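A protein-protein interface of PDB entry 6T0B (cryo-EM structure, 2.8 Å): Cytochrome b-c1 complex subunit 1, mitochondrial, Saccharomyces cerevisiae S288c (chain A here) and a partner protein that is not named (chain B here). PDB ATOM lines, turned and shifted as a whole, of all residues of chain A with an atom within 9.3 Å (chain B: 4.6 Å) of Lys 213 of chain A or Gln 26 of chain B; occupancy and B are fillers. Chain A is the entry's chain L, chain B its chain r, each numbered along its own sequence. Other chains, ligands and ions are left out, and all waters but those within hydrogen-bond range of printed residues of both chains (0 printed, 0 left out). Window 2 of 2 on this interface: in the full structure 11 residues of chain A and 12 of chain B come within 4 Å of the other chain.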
ATOM      1  N   ALA A  34      -1.517  -8.586  -2.760  1.00  0.00           N
ATOM      2  CA  ALA A  34      -1.483  -8.369  -1.324  1.00  0.00           C
ATOM      3  C   ALA A  34      -2.095  -7.043  -0.912  1.00  0.00           C
ATOM      4  O   ALA A  34      -2.046  -6.701   0.268  1.00  0.00           O
ATOM      5  CB  ALA A  34      -0.046  -8.433  -0.816  1.00  0.00           C
ATOM      6  N   ASN A  35      -2.642  -6.276  -1.842  1.00  0.00           N
ATOM      7  CA  ASN A  35      -3.258  -4.997  -1.540  1.00  0.00           C
ATOM      8  C   ASN A  35      -4.719  -5.009  -1.928  1.00  0.00           C
ATOM      9  O   ASN A  35      -5.260  -4.020  -2.411  1.00  0.00           O
ATOM     10  CB  ASN A  35      -2.533  -3.863  -2.246  1.00  0.00           C
ATOM     11  CG  ASN A  35      -1.105  -3.757  -1.834  1.00  0.00           C
ATOM     12  OD1 ASN A  35      -0.278  -4.558  -2.232  1.00  0.00           O
ATOM     13  ND2 ASN A  35      -0.801  -2.771  -1.015  1.00  0.00           N
ATOM     14  N   ASN A 145      -6.395 -14.636   6.920  1.00  0.00           N
ATOM     15  CA  ASN A 145      -6.960 -13.381   7.418  1.00  0.00           C
ATOM     16  C   ASN A 145      -5.960 -12.226   7.444  1.00  0.00           C
ATOM     17  O   ASN A 145      -6.217 -11.199   8.070  1.00  0.00           O
ATOM     18  CB  ASN A 145      -7.603 -13.559   8.794  1.00  0.00           C
ATOM     19  CG  ASN A 145      -8.644 -14.635   8.801  1.00  0.00           C
ATOM     20  OD1 ASN A 145      -8.722 -15.434   9.727  1.00  0.00           O
ATOM     21  ND2 ASN A 145      -9.452 -14.673   7.760  1.00  0.00           N
ATOM     22  N   THR A 146      -4.826 -12.361   6.776  1.00  0.00           N
ATOM     23  CA  THR A 146      -3.841 -11.317   6.557  1.00  0.00           C
ATOM     24  C   THR A 146      -3.703 -11.144   5.048  1.00  0.00           C
ATOM     25  O   THR A 146      -4.097 -12.045   4.302  1.00  0.00           O
ATOM     26  CB  THR A 146      -2.504 -11.697   7.215  1.00  0.00           C
ATOM     27  OG1 THR A 146      -1.871 -12.732   6.466  1.00  0.00           O
ATOM     28  CG2 THR A 146      -2.699 -12.135   8.643  1.00  0.00           C
ATOM     29  N   PRO A 147      -3.201 -10.000   4.547  1.00  0.00           N
ATOM     30  CA  PRO A 147      -3.357  -9.716   3.109  1.00  0.00           C
ATOM     31  C   PRO A 147      -2.539 -10.590   2.181  1.00  0.00           C
ATOM     32  O   PRO A 147      -2.828 -10.618   0.983  1.00  0.00           O
ATOM     33  CB  PRO A 147      -2.910  -8.259   2.993  1.00  0.00           C
ATOM     34  CG  PRO A 147      -3.021  -7.722   4.323  1.00  0.00           C
ATOM     35  CD  PRO A 147      -2.609  -8.819   5.201  1.00  0.00           C
ATOM     36  N   ASN A 173      -6.360   4.343  -6.442  1.00  0.00           N
ATOM     37  CA  ASN A 173      -5.700   4.139  -5.165  1.00  0.00           C
ATOM     38  C   ASN A 173      -4.274   3.641  -5.290  1.00  0.00           C
ATOM     39  O   ASN A 173      -3.501   3.810  -4.346  1.00  0.00           O
ATOM     40  CB  ASN A 173      -6.497   3.164  -4.314  1.00  0.00           C
ATOM     41  CG  ASN A 173      -7.630   3.832  -3.603  1.00  0.00           C
ATOM     42  OD1 ASN A 173      -8.723   3.288  -3.500  1.00  0.00           O
ATOM     43  ND2 ASN A 173      -7.385   5.035  -3.118  1.00  0.00           N
ATOM     44  N   PRO A 210      -2.998   3.546   0.056  1.00  0.00           N
ATOM     45  CA  PRO A 210      -3.392   3.279   1.439  1.00  0.00           C
ATOM     46  C   PRO A 210      -2.481   2.256   2.084  1.00  0.00           C
ATOM     47  O   PRO A 210      -2.072   1.282   1.454  1.00  0.00           O
ATOM     48  CB  PRO A 210      -4.819   2.747   1.302  1.00  0.00           C
ATOM     49  CG  PRO A 210      -4.894   2.251  -0.065  1.00  0.00           C
ATOM     50  CD  PRO A 210      -4.071   3.187  -0.874  1.00  0.00           C
ATOM     51  N   VAL A 211      -2.162   2.486   3.352  1.00  0.00           N
ATOM     52  CA  VAL A 211      -1.266   1.615   4.096  1.00  0.00           C
ATOM     53  C   VAL A 211      -2.101   0.589   4.854  1.00  0.00           C
ATOM     54  O   VAL A 211      -3.107   0.928   5.487  1.00  0.00           O
ATOM     55  CB  VAL A 211      -0.328   2.428   5.012  1.00  0.00           C
ATOM     56  CG1 VAL A 211      -1.077   3.297   6.013  1.00  0.00           C
ATOM     57  CG2 VAL A 211       0.663   1.521   5.712  1.00  0.00           C
ATOM     58  N   LEU A 212      -1.721  -0.679   4.734  1.00  0.00           N
ATOM     59  CA  LEU A 212      -2.565  -1.761   5.217  1.00  0.00           C
ATOM     60  C   LEU A 212      -2.500  -1.867   6.730  1.00  0.00           C
ATOM     61  O   LEU A 212      -1.434  -1.746   7.334  1.00  0.00           O
ATOM     62  CB  LEU A 212      -2.141  -3.078   4.587  1.00  0.00           C
ATOM     63  CG  LEU A 212      -2.418  -3.220   3.101  1.00  0.00           C
ATOM     64  CD1 LEU A 212      -1.441  -4.200   2.519  1.00  0.00           C
ATOM     65  CD2 LEU A 212      -3.838  -3.685   2.885  1.00  0.00           C
ATOM     66  N   LYS A 213      -3.652  -2.123   7.342  1.00  0.00           N
ATOM     67  CA  LYS A 213      -3.753  -2.028   8.787  1.00  0.00           C
ATOM     68  C   LYS A 213      -3.180  -3.229   9.522  1.00  0.00           C
ATOM     69  O   LYS A 213      -3.015  -3.155  10.742  1.00  0.00           O
ATOM     70  CB  LYS A 213      -5.208  -1.827   9.197  1.00  0.00           C
ATOM     71  CG  LYS A 213      -5.539  -0.385   9.502  1.00  0.00           C
ATOM     72  CD  LYS A 213      -6.628  -0.257  10.545  1.00  0.00           C
ATOM     73  CE  LYS A 213      -6.917   1.208  10.825  1.00  0.00           C
ATOM     74  NZ  LYS A 213      -8.275   1.436  11.388  1.00  0.00           N
ATOM     75  N   LYS A 214      -2.873  -4.326   8.835  1.00  0.00           N
ATOM     76  CA  LYS A 214      -2.285  -5.477   9.501  1.00  0.00           C
ATOM     77  C   LYS A 214      -1.213  -6.095   8.625  1.00  0.00           C
ATOM     78  O   LYS A 214      -1.342  -6.148   7.403  1.00  0.00           O
ATOM     79  CB  LYS A 214      -3.328  -6.535   9.843  1.00  0.00           C
ATOM     80  CG  LYS A 214      -4.272  -6.845   8.722  1.00  0.00           C
ATOM     81  CD  LYS A 214      -4.944  -8.181   8.943  1.00  0.00           C
ATOM     82  CE  LYS A 214      -5.619  -8.250  10.296  1.00  0.00           C
ATOM     83  NZ  LYS A 214      -6.512  -9.428  10.408  1.00  0.00           N
ATOM     84  N   LYS A 215      -0.157  -6.564   9.267  1.00  0.00           N
ATOM     85  CA  LYS A 215       0.925  -7.233   8.569  1.00  0.00           C
ATOM     86  C   LYS A 215       0.626  -8.717   8.451  1.00  0.00           C
ATOM     87  O   LYS A 215      -0.216  -9.263   9.162  1.00  0.00           O
ATOM     88  CB  LYS A 215       2.245  -7.026   9.296  1.00  0.00           C
ATOM     89  CG  LYS A 215       2.740  -5.602   9.271  1.00  0.00           C
ATOM     90  CD  LYS A 215       4.015  -5.463  10.071  1.00  0.00           C
ATOM     91  CE  LYS A 215       5.169  -6.154   9.370  1.00  0.00           C
ATOM     92  NZ  LYS A 215       5.533  -5.461   8.105  1.00  0.00           N
ATOM     93  N   ALA A 216       1.337  -9.368   7.538  1.00  0.00           N
ATOM     94  CA  ALA A 216       1.124 -10.785   7.292  1.00  0.00           C
ATOM     95  C   ALA A 216       1.751 -11.606   8.403  1.00  0.00           C
ATOM     96  O   ALA A 216       2.939 -11.460   8.702  1.00  0.00           O
ATOM     97  CB  ALA A 216       1.708 -11.175   5.944  1.00  0.00           C
ATOM     98  N   TRP B  18     -14.952  -3.317   8.554  1.00  0.00           N
ATOM     99  CA  TRP B  18     -14.749  -1.883   8.695  1.00  0.00           C
ATOM    100  C   TRP B  18     -13.536  -1.522   9.557  1.00  0.00           C
ATOM    101  O   TRP B  18     -13.017  -0.411   9.440  1.00  0.00           O
ATOM    102  CB  TRP B  18     -16.035  -1.262   9.256  1.00  0.00           C
ATOM    103  CG  TRP B  18     -15.920   0.155   9.666  1.00  0.00           C
ATOM    104  CD1 TRP B  18     -15.615   0.622  10.901  1.00  0.00           C
ATOM    105  CD2 TRP B  18     -16.057   1.298   8.829  1.00  0.00           C
ATOM    106  NE1 TRP B  18     -15.564   1.988  10.893  1.00  0.00           N
ATOM    107  CE2 TRP B  18     -15.833   2.428   9.628  1.00  0.00           C
ATOM    108  CE3 TRP B  18     -16.358   1.477   7.484  1.00  0.00           C
ATOM    109  CZ2 TRP B  18     -15.904   3.717   9.126  1.00  0.00           C
ATOM    110  CZ3 TRP B  18     -16.425   2.752   6.991  1.00  0.00           C
ATOM    111  CH2 TRP B  18     -16.198   3.856   7.805  1.00  0.00           C
ATOM    112  N   GLU B  19     -13.057  -2.414  10.415  1.00  0.00           N
ATOM    113  CA  GLU B  19     -11.955  -2.045  11.297  1.00  0.00           C
ATOM    114  C   GLU B  19     -10.612  -2.592  10.853  1.00  0.00           C
ATOM    115  O   GLU B  19      -9.581  -1.987  11.158  1.00  0.00           O
ATOM    116  CB  GLU B  19     -12.249  -2.500  12.727  1.00  0.00           C
ATOM    117  CG  GLU B  19     -13.352  -1.700  13.409  1.00  0.00           C
ATOM    118  CD  GLU B  19     -14.750  -2.252  13.155  1.00  0.00           C
ATOM    119  OE1 GLU B  19     -15.022  -2.777  12.054  1.00  0.00           O
ATOM    120  OE2 GLU B  19     -15.586  -2.178  14.076  1.00  0.00           O
ATOM    121  N   ASN B  20     -10.595  -3.714  10.139  1.00  0.00           N
ATOM    122  CA  ASN B  20      -9.492  -4.035   9.240  1.00  0.00           C
ATOM    123  C   ASN B  20      -9.754  -3.239   7.963  1.00  0.00           C
ATOM    124  O   ASN B  20     -10.242  -3.747   6.952  1.00  0.00           O
ATOM    125  CB  ASN B  20      -9.415  -5.537   8.990  1.00  0.00           C
ATOM    126  CG  ASN B  20      -8.235  -5.957   8.091  1.00  0.00           C
ATOM    127  OD1 ASN B  20      -7.517  -5.135   7.508  1.00  0.00           O
ATOM    128  ND2 ASN B  20      -8.043  -7.267   7.977  1.00  0.00           N
ATOM    129  N   MET B  21      -9.416  -1.957   8.028  1.00  0.00           N
ATOM    130  CA  MET B  21      -9.618  -1.049   6.913  1.00  0.00           C
ATOM    131  C   MET B  21      -8.422  -0.113   6.868  1.00  0.00           C
ATOM    132  O   MET B  21      -8.193   0.636   7.835  1.00  0.00           O
ATOM    133  CB  MET B  21     -10.917  -0.264   7.053  1.00  0.00           C
ATOM    134  CG  MET B  21     -11.378   0.360   5.777  1.00  0.00           C
ATOM    135  SD  MET B  21     -11.868  -0.866   4.559  1.00  0.00           S
ATOM    136  CE  MET B  21     -13.600  -1.061   4.930  1.00  0.00           C
ATOM    137  N   PRO B  22      -7.678  -0.080   5.770  1.00  0.00           N
ATOM    138  CA  PRO B  22      -6.492   0.781   5.652  1.00  0.00           C
ATOM    139  C   PRO B  22      -6.619   2.293   5.843  1.00  0.00           C
ATOM    140  O   PRO B  22      -5.657   3.011   5.554  1.00  0.00           O
ATOM    141  CB  PRO B  22      -6.034   0.466   4.228  1.00  0.00           C
ATOM    142  CG  PRO B  22      -6.369  -1.000   4.066  1.00  0.00           C
ATOM    143  CD  PRO B  22      -7.452  -1.351   5.063  1.00  0.00           C
ATOM    144  N   ASN B  23      -7.791   2.792   6.239  1.00  0.00           N
ATOM    145  CA  ASN B  23      -8.067   4.072   6.885  1.00  0.00           C
ATOM    146  C   ASN B  23      -8.042   5.252   5.921  1.00  0.00           C
ATOM    147  O   ASN B  23      -8.553   6.313   6.266  1.00  0.00           O
ATOM    148  CB  ASN B  23      -7.100   4.363   8.054  1.00  0.00           C
ATOM    149  CG  ASN B  23      -7.603   5.428   8.985  1.00  0.00           C
ATOM    150  OD1 ASN B  23      -8.804   5.619   9.132  1.00  0.00           O
ATOM    151  ND2 ASN B  23      -6.682   6.149   9.607  1.00  0.00           N
ATOM    152  N   LEU B  24      -7.549   5.093   4.702  1.00  0.00           N
ATOM    153  CA  LEU B  24      -7.767   6.140   3.720  1.00  0.00           C
ATOM    154  C   LEU B  24      -9.150   5.993   3.119  1.00  0.00           C
ATOM    155  O   LEU B  24      -9.885   6.974   2.966  1.00  0.00           O
ATOM    156  CB  LEU B  24      -6.699   6.078   2.636  1.00  0.00           C
ATOM    157  CG  LEU B  24      -7.009   6.890   1.385  1.00  0.00           C
ATOM    158  CD1 LEU B  24      -6.942   8.375   1.689  1.00  0.00           C
ATOM    159  CD2 LEU B  24      -6.068   6.518   0.259  1.00  0.00           C
ATOM    160  N   GLU B  25      -9.532   4.757   2.825  1.00  0.00           N
ATOM    161  CA  GLU B  25     -10.794   4.441   2.183  1.00  0.00           C
ATOM    162  C   GLU B  25     -11.974   4.466   3.131  1.00  0.00           C
ATOM    163  O   GLU B  25     -13.110   4.379   2.662  1.00  0.00           O
ATOM    164  CB  GLU B  25     -10.704   3.072   1.525  1.00  0.00           C
ATOM    165  CG  GLU B  25     -10.796   1.947   2.498  1.00  0.00           C
ATOM    166  CD  GLU B  25      -9.474   1.611   3.153  1.00  0.00           C
ATOM    167  OE1 GLU B  25      -8.821   2.486   3.763  1.00  0.00           O
ATOM    168  OE2 GLU B  25      -9.096   0.442   3.044  1.00  0.00           O
ATOM    169  N   GLN B  26     -11.740   4.549   4.441  1.00  0.00           N
ATOM    170  CA  GLN B  26     -12.823   4.889   5.354  1.00  0.00           C
ATOM    171  C   GLN B  26     -13.381   6.266   5.023  1.00  0.00           C
ATOM    172  O   GLN B  26     -14.600   6.474   5.023  1.00  0.00           O
ATOM    173  CB  GLN B  26     -12.322   4.833   6.794  1.00  0.00           C
ATOM    174  CG  GLN B  26     -12.469   3.482   7.457  1.00  0.00           C
ATOM    175  CD  GLN B  26     -12.078   3.512   8.911  1.00  0.00           C
ATOM    176  OE1 GLN B  26     -12.168   4.544   9.561  1.00  0.00           O
ATOM    177  NE2 GLN B  26     -11.624   2.380   9.426  1.00  0.00           N
ATOM    178  N   LYS B  27     -12.501   7.196   4.660  1.00  0.00           N
ATOM    179  CA  LYS B  27     -12.922   8.541   4.292  1.00  0.00           C
ATOM    180  C   LYS B  27     -13.628   8.541   2.942  1.00  0.00           C
ATOM    181  O   LYS B  27     -14.728   9.100   2.804  1.00  0.00           O
ATOM    182  CB  LYS B  27     -11.720   9.486   4.276  1.00  0.00           C
ATOM    183  CG  LYS B  27     -11.310  10.032   5.644  1.00  0.00           C
ATOM    184  CD  LYS B  27     -10.542   9.009   6.469  1.00  0.00           C
ATOM    185  CE  LYS B  27     -10.165   9.518   7.842  1.00  0.00           C
ATOM    186  NZ  LYS B  27      -9.592   8.417   8.661  1.00  0.00           N
ATOM    187  N   GLU B  28     -13.028   7.893   1.938  1.00  0.00           N
ATOM    188  CA  GLU B  28     -13.680   7.819   0.639  1.00  0.00           C
ATOM    189  C   GLU B  28     -14.713   6.707   0.561  1.00  0.00           C
ATOM    190  O   GLU B  28     -15.113   6.332  -0.542  1.00  0.00           O
ATOM    191  CB  GLU B  28     -12.661   7.704  -0.507  1.00  0.00           C
ATOM    192  CG  GLU B  28     -11.867   6.423  -0.634  1.00  0.00           C
ATOM    193  CD  GLU B  28     -10.818   6.488  -1.735  1.00  0.00           C
ATOM    194  OE1 GLU B  28     -10.723   7.530  -2.415  1.00  0.00           O
ATOM    195  OE2 GLU B  28     -10.071   5.503  -1.903  1.00  0.00           O
ATOM    196  N   ILE B  29     -15.169   6.186   1.694  1.00  0.00           N
ATOM    197  CA  ILE B  29     -16.450   5.502   1.753  1.00  0.00           C
ATOM    198  C   ILE B  29     -17.450   6.221   2.663  1.00  0.00           C
ATOM    199  O   ILE B  29     -18.660   5.973   2.552  1.00  0.00           O
ATOM    200  CB  ILE B  29     -16.273   4.025   2.167  1.00  0.00           C
ATOM    201  CG1 ILE B  29     -17.476   3.190   1.744  1.00  0.00           C
ATOM    202  CG2 ILE B  29     -16.140   3.903   3.647  1.00  0.00           C
ATOM    203  CD1 ILE B  29     -17.853   3.413   0.320  1.00  0.00           C
ATOM    204  N   ALA B  30     -17.006   7.134   3.521  1.00  0.00           N
ATOM    205  CA  ALA B  30     -17.983   7.916   4.264  1.00  0.00           C
ATOM    206  C   ALA B  30     -18.571   9.016   3.395  1.00  0.00           C
ATOM    207  O   ALA B  30     -19.785   9.277   3.444  1.00  0.00           O
ATOM    208  CB  ALA B  30     -17.350   8.504   5.518  1.00  0.00           C
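ND2 of Asn 173 of chain A touches CD2 of Leu 24 of chain B, 3.9 Å away. Pro 22 of chain B touches Pro 210 of chain A (CB to CB, 3.9 Å). Pro 22 of chain B touches Leu 212 of chain A (CG to CD2, 3.9 Å). Lys 213 of chain A touches Glu 19 of chain B (CD to O, 3.5 Å). Lys 213 of chain A touches Met 21 of chain B (CD to O, 3.3 Å). NZ of Lys 213 of chain A touches NE2 of Gln 26 of chain B, 3.99 Å away. Lys 214 of chain A touches Asn 20 of chain B (CD to ND2, 3.4 Å).
The side-chain carboxylate (OE2) of Glu 28 of chain B sits at hydrogen-bond distance from the side-chain amide nitrogen (ND2) of Asn 173 of chain A (3.0 Å). O of Val 211 of chain A lies close to O of Pro 22 of chain B, 3.3 Å away.
The backbone carbonyl oxygen (O) of Asn 145 of chain A is in hydrogen-bond range of the side-chain amino group (NZ) of Lys 214 of chain A (2.9 Å). The side-chain amide nitrogen of Gln 26 of chain B sits at hydrogen-bond distance from the backbone carbonyl oxygen of Trp 18 of chain B (3.1 Å).
Of the 13 printed residues of chain A, 6 touch a printed residue of chain B. Printed residues of chain A that touch a printed residue of chain B: Asn 173, Pro 210, Val 211, Leu 212, Lys 213 and Lys 214. Hydrophobic or aromatic side chains of chain B within 4 Å of the printed part of chain A: Pro 22 and Leu 24. Among the printed residues, 9 pairs touch across the chains. Among the printed residues, no Asp or Glu carboxylate lies within 4 Å of a Lys or Arg side-chain nitrogen of the other chain.
Asn 35 of chain A touches none of the printed residues of chain B. Asn 145 of chain A touches none of the printed residues of chain B. Of the printed residues of chain B, Asn 173 of chain A touches Leu 24 and Glu 28. Printed residues of chain B within 4 Å of Val 211 of chain A: Pro 22. Of the printed residues of chain B, Lys 213 of chain A touches Glu 19 (3.5 Å), Met 21 (3.3 Å) and Gln 26 (3.99 Å). Printed residues of chain B within 4 Å of Lys 214 of chain A: Asn 20. Printed residues of chain A within 4 Å of Glu 19 of chain B: Lys 213 (3.5 Å). Of the printed residues of chain A, Pro 22 of chain B touches Pro 210 (3.9 Å), Val 211 (3.2 Å) and Leu 212 (3.9 Å). Asn 23 of chain B touches none of the printed residues of chain A. Of the printed residues of chain A, Gln 26 of chain B touches Lys 213. The nearest printed residue of chain A that does not touch Gln 26 of chain B is Pro 210 of chain A (7.8 Å). The nearest printed residue of chain B that does not touch Lys 214 of chain A is Pro 22 of chain B (6.6 Å).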
